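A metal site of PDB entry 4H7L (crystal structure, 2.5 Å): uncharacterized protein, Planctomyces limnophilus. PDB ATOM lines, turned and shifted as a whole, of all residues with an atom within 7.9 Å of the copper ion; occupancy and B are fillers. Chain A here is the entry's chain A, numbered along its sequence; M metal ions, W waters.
O of His 61 lies within hydrogen-bond range of N of His 104, 2.9 Å away.
OE1 of Glu 68 sits close to OH of Tyr 70 (3.2 Å).
The side-chain amide nitrogen (ND2) of Asn 114 is in hydrogen-bond range of the side-chain carboxylate (OE2) of Glu 68.
OE1 of Glu 68 sits close to NE2 of His 104, 3.3 Å away.
The backbone NH (N) of Ile 98 sits at hydrogen-bond distance from the backbone carbonyl oxygen (O) of Glu 68.
NE2 of His 104 lies close to OH of Tyr 70 (3.4 Å).
A ring nitrogen (ND1) of His 63 sits at hydrogen-bond distance from the backbone carbonyl oxygen (O) of Asp 124 (3.0 Å).
A ring nitrogen (ND1) of His 104 lies within hydrogen-bond range of the backbone carbonyl oxygen (O) of Val 102 (2.6 Å).
Merely in contact with the copper ion: Tyr 70.
Within 4 Å of the copper ion: His 61, His 63, Glu 68, Tyr 70 and His 104.
The copper ion is bound by OE1 of Glu 68 (2.2 Å).
A ring nitrogen (NE2) of His 61 is bound to the copper ion, at 2.2 Å.
NE2 of His 63 is bound to the copper ion, at 2.2 Å.
Water W1 is bound to the copper ion (2.4 Å).
The copper ion has four donor atoms within binding distance.
Slightly farther from the copper ion lies a ring nitrogen (NE2) of His 104 (2.6 Å).
Water W1 bridges the side-chain hydroxyl of Tyr 70 (2.9 Å) and the side-chain carboxylate of Glu 68 (3.5 Å).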
ATOM      1  N   CYS A  32     -31.693  27.623   9.253  1.00  0.00           N
ATOM      2  CA  CYS A  32     -31.906  26.331   8.607  1.00  0.00           C
ATOM      3  C   CYS A  32     -33.292  25.754   8.862  1.00  0.00           C
ATOM      4  O   CYS A  32     -33.735  24.845   8.162  1.00  0.00           O
ATOM      5  CB  CYS A  32     -30.835  25.342   9.059  1.00  0.00           C
ATOM      6  SG  CYS A  32     -30.853  25.018  10.825  1.00  0.00           S
ATOM      7  N   HIS A  61     -22.474  28.125   7.034  1.00  0.00           N
ATOM      8  CA  HIS A  61     -22.059  28.868   8.217  1.00  0.00           C
ATOM      9  C   HIS A  61     -20.932  28.152   8.960  1.00  0.00           C
ATOM     10  O   HIS A  61     -20.637  26.988   8.695  1.00  0.00           O
ATOM     11  CB  HIS A  61     -23.261  29.102   9.156  1.00  0.00           C
ATOM     12  CG  HIS A  61     -23.592  27.922  10.020  1.00  0.00           C
ATOM     13  ND1 HIS A  61     -24.427  26.907   9.600  1.00  0.00           N
ATOM     14  CD2 HIS A  61     -23.232  27.610  11.284  1.00  0.00           C
ATOM     15  CE1 HIS A  61     -24.540  26.009  10.569  1.00  0.00           C
ATOM     16  NE2 HIS A  61     -23.826  26.419  11.604  1.00  0.00           N
ATOM     17  N   TYR A  62     -20.292  28.860   9.889  1.00  0.00           N
ATOM     18  CA  TYR A  62     -19.292  28.255  10.750  1.00  0.00           C
ATOM     19  C   TYR A  62     -19.213  28.948  12.118  1.00  0.00           C
ATOM     20  O   TYR A  62     -19.677  30.081  12.281  1.00  0.00           O
ATOM     21  CB  TYR A  62     -17.917  28.240  10.083  1.00  0.00           C
ATOM     22  CG  TYR A  62     -17.244  29.601   9.947  1.00  0.00           C
ATOM     23  CD1 TYR A  62     -17.505  30.426   8.861  1.00  0.00           C
ATOM     24  CD2 TYR A  62     -16.342  30.040  10.905  1.00  0.00           C
ATOM     25  CE1 TYR A  62     -16.880  31.659   8.739  1.00  0.00           C
ATOM     26  CE2 TYR A  62     -15.717  31.273  10.783  1.00  0.00           C
ATOM     27  CZ  TYR A  62     -15.989  32.070   9.696  1.00  0.00           C
ATOM     28  OH  TYR A  62     -15.377  33.297   9.572  1.00  0.00           O
ATOM     29  N   HIS A  63     -18.625  28.250  13.087  1.00  0.00           N
ATOM     30  CA  HIS A  63     -18.533  28.741  14.459  1.00  0.00           C
ATOM     31  C   HIS A  63     -17.060  28.920  14.818  1.00  0.00           C
ATOM     32  O   HIS A  63     -16.227  28.095  14.461  1.00  0.00           O
ATOM     33  CB  HIS A  63     -19.208  27.756  15.414  1.00  0.00           C
ATOM     34  CG  HIS A  63     -20.518  27.240  14.909  1.00  0.00           C
ATOM     35  ND1 HIS A  63     -21.678  27.996  14.920  1.00  0.00           N
ATOM     36  CD2 HIS A  63     -20.867  26.044  14.377  1.00  0.00           C
ATOM     37  CE1 HIS A  63     -22.671  27.290  14.415  1.00  0.00           C
ATOM     38  NE2 HIS A  63     -22.211  26.100  14.072  1.00  0.00           N
ATOM     39  N   HIS A  66     -16.930  27.074  19.012  1.00  0.00           N
ATOM     40  CA  HIS A  66     -17.829  26.008  19.407  1.00  0.00           C
ATOM     41  C   HIS A  66     -17.662  24.738  18.580  1.00  0.00           C
ATOM     42  O   HIS A  66     -17.647  24.785  17.351  1.00  0.00           O
ATOM     43  CB  HIS A  66     -19.275  26.491  19.334  1.00  0.00           C
ATOM     44  CG  HIS A  66     -19.655  27.430  20.433  1.00  0.00           C
ATOM     45  ND1 HIS A  66     -19.614  28.801  20.272  1.00  0.00           N
ATOM     46  CD2 HIS A  66     -20.069  27.204  21.699  1.00  0.00           C
ATOM     47  CE1 HIS A  66     -19.993  29.377  21.400  1.00  0.00           C
ATOM     48  NE2 HIS A  66     -20.264  28.436  22.285  1.00  0.00           N
ATOM     49  N   GLN A  67     -17.514  23.614  19.265  1.00  0.00           N
ATOM     50  CA  GLN A  67     -17.568  22.311  18.626  1.00  0.00           C
ATOM     51  C   GLN A  67     -19.033  21.927  18.491  1.00  0.00           C
ATOM     52  O   GLN A  67     -19.819  22.188  19.391  1.00  0.00           O
ATOM     53  CB  GLN A  67     -16.862  21.250  19.465  1.00  0.00           C
ATOM     54  CG  GLN A  67     -15.362  21.449  19.623  1.00  0.00           C
ATOM     55  CD  GLN A  67     -14.716  20.288  20.336  1.00  0.00           C
ATOM     56  OE1 GLN A  67     -15.312  19.220  20.486  1.00  0.00           O
ATOM     57  NE2 GLN A  67     -13.485  20.484  20.803  1.00  0.00           N
ATOM     58  N   GLU A  68     -19.383  21.306  17.375  1.00  0.00           N
ATOM     59  CA  GLU A  68     -20.731  20.781  17.201  1.00  0.00           C
ATOM     60  C   GLU A  68     -20.667  19.311  16.818  1.00  0.00           C
ATOM     61  O   GLU A  68     -19.786  18.894  16.075  1.00  0.00           O
ATOM     62  CB  GLU A  68     -21.506  21.563  16.137  1.00  0.00           C
ATOM     63  CG  GLU A  68     -21.984  22.930  16.616  1.00  0.00           C
ATOM     64  CD  GLU A  68     -22.945  23.599  15.648  1.00  0.00           C
ATOM     65  OE1 GLU A  68     -22.886  23.295  14.434  1.00  0.00           O
ATOM     66  OE2 GLU A  68     -23.762  24.436  16.097  1.00  0.00           O
ATOM     67  N   ILE A  69     -21.615  18.536  17.342  1.00  0.00           N
ATOM     68  CA  ILE A  69     -21.808  17.169  16.886  1.00  0.00           C
ATOM     69  C   ILE A  69     -23.255  16.999  16.462  1.00  0.00           C
ATOM     70  O   ILE A  69     -24.158  17.157  17.273  1.00  0.00           O
ATOM     71  CB  ILE A  69     -21.496  16.123  17.984  1.00  0.00           C
ATOM     72  CG1 ILE A  69     -20.043  16.253  18.432  1.00  0.00           C
ATOM     73  CG2 ILE A  69     -21.774  14.717  17.459  1.00  0.00           C
ATOM     74  CD1 ILE A  69     -19.658  15.257  19.514  1.00  0.00           C
ATOM     75  N   TYR A  70     -23.473  16.694  15.188  1.00  0.00           N
ATOM     76  CA  TYR A  70     -24.810  16.387  14.704  1.00  0.00           C
ATOM     77  C   TYR A  70     -25.063  14.889  14.824  1.00  0.00           C
ATOM     78  O   TYR A  70     -24.191  14.081  14.537  1.00  0.00           O
ATOM     79  CB  TYR A  70     -24.979  16.772  13.235  1.00  0.00           C
ATOM     80  CG  TYR A  70     -24.939  18.252  12.945  1.00  0.00           C
ATOM     81  CD1 TYR A  70     -24.759  19.196  13.958  1.00  0.00           C
ATOM     82  CD2 TYR A  70     -25.096  18.713  11.647  1.00  0.00           C
ATOM     83  CE1 TYR A  70     -24.727  20.546  13.672  1.00  0.00           C
ATOM     84  CE2 TYR A  70     -25.071  20.062  11.354  1.00  0.00           C
ATOM     85  CZ  TYR A  70     -24.878  20.975  12.372  1.00  0.00           C
ATOM     86  OH  TYR A  70     -24.853  22.320  12.093  1.00  0.00           O
ATOM     87  N   ILE A  98     -18.051  18.420  14.138  1.00  0.00           N
ATOM     88  CA  ILE A  98     -17.749  19.598  13.340  1.00  0.00           C
ATOM     89  C   ILE A  98     -16.956  20.571  14.192  1.00  0.00           C
ATOM     90  O   ILE A  98     -17.517  21.342  14.956  1.00  0.00           O
ATOM     91  CB  ILE A  98     -19.048  20.258  12.851  1.00  0.00           C
ATOM     92  CG1 ILE A  98     -19.872  19.254  12.057  1.00  0.00           C
ATOM     93  CG2 ILE A  98     -18.723  21.487  12.002  1.00  0.00           C
ATOM     94  CD1 ILE A  98     -21.262  19.726  11.704  1.00  0.00           C
ATOM     95  N   VAL A 102     -14.939  24.940  10.720  1.00  0.00           N
ATOM     96  CA  VAL A 102     -15.358  24.117   9.602  1.00  0.00           C
ATOM     97  C   VAL A 102     -16.645  24.681   9.001  1.00  0.00           C
ATOM     98  O   VAL A 102     -17.683  24.705   9.648  1.00  0.00           O
ATOM     99  CB  VAL A 102     -15.595  22.653  10.028  1.00  0.00           C
ATOM    100  CG1 VAL A 102     -16.343  21.890   8.943  1.00  0.00           C
ATOM    101  CG2 VAL A 102     -14.275  21.968  10.338  1.00  0.00           C
ATOM    102  N   HIS A 104     -19.987  24.692   7.006  1.00  0.00           N
ATOM    103  CA  HIS A 104     -20.912  23.578   6.876  1.00  0.00           C
ATOM    104  C   HIS A 104     -22.379  23.984   6.801  1.00  0.00           C
ATOM    105  O   HIS A 104     -22.775  25.065   7.257  1.00  0.00           O
ATOM    106  CB  HIS A 104     -20.735  22.615   8.062  1.00  0.00           C
ATOM    107  CG  HIS A 104     -21.066  23.229   9.386  1.00  0.00           C
ATOM    108  ND1 HIS A 104     -20.170  24.008  10.094  1.00  0.00           N
ATOM    109  CD2 HIS A 104     -22.191  23.155  10.146  1.00  0.00           C
ATOM    110  CE1 HIS A 104     -20.734  24.397  11.227  1.00  0.00           C
ATOM    111  NE2 HIS A 104     -21.950  23.903  11.282  1.00  0.00           N
ATOM    112  N   ARG A 105     -23.180  23.093   6.219  1.00  0.00           N
ATOM    113  CA  ARG A 105     -24.625  23.215   6.241  1.00  0.00           C
ATOM    114  C   ARG A 105     -25.255  21.891   5.824  1.00  0.00           C
ATOM    115  O   ARG A 105     -24.564  20.991   5.358  1.00  0.00           O
ATOM    116  CB  ARG A 105     -25.103  24.311   5.288  1.00  0.00           C
ATOM    117  CG  ARG A 105     -24.717  24.056   3.845  1.00  0.00           C
ATOM    118  CD  ARG A 105     -25.543  24.909   2.915  1.00  0.00           C
ATOM    119  NE  ARG A 105     -25.087  24.804   1.531  1.00  0.00           N
ATOM    120  CZ  ARG A 105     -25.430  25.635   0.561  1.00  0.00           C
ATOM    121  NH1 ARG A 105     -26.247  26.652   0.807  1.00  0.00           N
ATOM    122  NH2 ARG A 105     -24.969  25.458  -0.661  1.00  0.00           N
ATOM    123  N   ILE A 112     -32.293  16.596  13.287  1.00  0.00           N
ATOM    124  CA  ILE A 112     -31.061  16.250  13.986  1.00  0.00           C
ATOM    125  C   ILE A 112     -31.098  16.583  15.460  1.00  0.00           C
ATOM    126  O   ILE A 112     -31.931  17.365  15.915  1.00  0.00           O
ATOM    127  CB  ILE A 112     -29.837  16.989  13.392  1.00  0.00           C
ATOM    128  CG1 ILE A 112     -29.955  18.496  13.618  1.00  0.00           C
ATOM    129  CG2 ILE A 112     -29.681  16.668  11.905  1.00  0.00           C
ATOM    130  CD1 ILE A 112     -28.737  19.287  13.174  1.00  0.00           C
ATOM    131  N   ASN A 114     -28.484  18.373  17.801  1.00  0.00           N
ATOM    132  CA  ASN A 114     -27.248  19.154  17.731  1.00  0.00           C
ATOM    133  C   ASN A 114     -26.623  19.382  19.104  1.00  0.00           C
ATOM    134  O   ASN A 114     -27.188  20.069  19.946  1.00  0.00           O
ATOM    135  CB  ASN A 114     -27.497  20.486  17.039  1.00  0.00           C
ATOM    136  CG  ASN A 114     -26.231  21.318  16.925  1.00  0.00           C
ATOM    137  OD1 ASN A 114     -25.126  20.793  16.972  1.00  0.00           O
ATOM    138  ND2 ASN A 114     -26.407  22.630  16.788  1.00  0.00           N
ATOM    139  N   VAL A 116     -23.694  20.899  21.346  1.00  0.00           N
ATOM    140  CA  VAL A 116     -22.828  22.067  21.227  1.00  0.00           C
ATOM    141  C   VAL A 116     -21.908  22.217  22.436  1.00  0.00           C
ATOM    142  O   VAL A 116     -22.323  22.042  23.576  1.00  0.00           O
ATOM    143  CB  VAL A 116     -23.670  23.347  21.045  1.00  0.00           C
ATOM    144  CG1 VAL A 116     -22.786  24.529  20.693  1.00  0.00           C
ATOM    145  CG2 VAL A 116     -24.738  23.131  19.975  1.00  0.00           C
ATOM    146  N   PHE A 120     -24.249  26.539  23.810  1.00  0.00           N
ATOM    147  CA  PHE A 120     -24.616  27.356  22.672  1.00  0.00           C
ATOM    148  C   PHE A 120     -24.543  28.859  22.929  1.00  0.00           C
ATOM    149  O   PHE A 120     -24.970  29.345  23.986  1.00  0.00           O
ATOM    150  CB  PHE A 120     -26.029  26.978  22.235  1.00  0.00           C
ATOM    151  CG  PHE A 120     -26.567  27.815  21.115  1.00  0.00           C
ATOM    152  CD1 PHE A 120     -26.072  27.687  19.819  1.00  0.00           C
ATOM    153  CD2 PHE A 120     -27.612  28.700  21.348  1.00  0.00           C
ATOM    154  CE1 PHE A 120     -26.593  28.456  18.797  1.00  0.00           C
ATOM    155  CE2 PHE A 120     -28.126  29.473  20.319  1.00  0.00           C
ATOM    156  CZ  PHE A 120     -27.617  29.347  19.039  1.00  0.00           C
ATOM    157  N   ASP A 124     -22.172  33.353  18.065  1.00  0.00           N
ATOM    158  CA  ASP A 124     -21.144  32.636  17.321  1.00  0.00           C
ATOM    159  C   ASP A 124     -21.713  31.945  16.085  1.00  0.00           C
ATOM    160  O   ASP A 124     -21.986  30.743  16.104  1.00  0.00           O
ATOM    161  CB  ASP A 124     -20.447  31.617  18.233  1.00  0.00           C
ATOM    162  CG  ASP A 124     -19.154  31.096  17.640  1.00  0.00           C
ATOM    163  OD1 ASP A 124     -18.762  29.955  17.972  1.00  0.00           O
ATOM    164  OD2 ASP A 124     -18.522  31.826  16.851  1.00  0.00           O
ATOM    165  N   GLU A 125     -21.879  32.705  15.014  1.00  0.00           N
ATOM    166  CA  GLU A 125     -22.319  32.178  13.728  1.00  0.00           C
ATOM    167  C   GLU A 125     -21.776  33.089  12.642  1.00  0.00           C
ATOM    168  O   GLU A 125     -22.071  34.288  12.621  1.00  0.00           O
ATOM    169  CB  GLU A 125     -23.838  32.114  13.657  1.00  0.00           C
ATOM    170  CG  GLU A 125     -24.389  30.714  13.444  1.00  0.00           C
ATOM    171  CD  GLU A 125     -25.756  30.729  12.772  1.00  0.00           C
ATOM    172  OE1 GLU A 125     -26.216  29.649  12.330  1.00  0.00           O
ATOM    173  OE2 GLU A 125     -26.374  31.815  12.686  1.00  0.00           O
HETATM  174 CU    CU M   1     -23.684  24.751  13.053  1.00  0.00          CU
HETATM  175  O   HOH W   1     -26.054  24.550  13.501  1.00  0.00           O
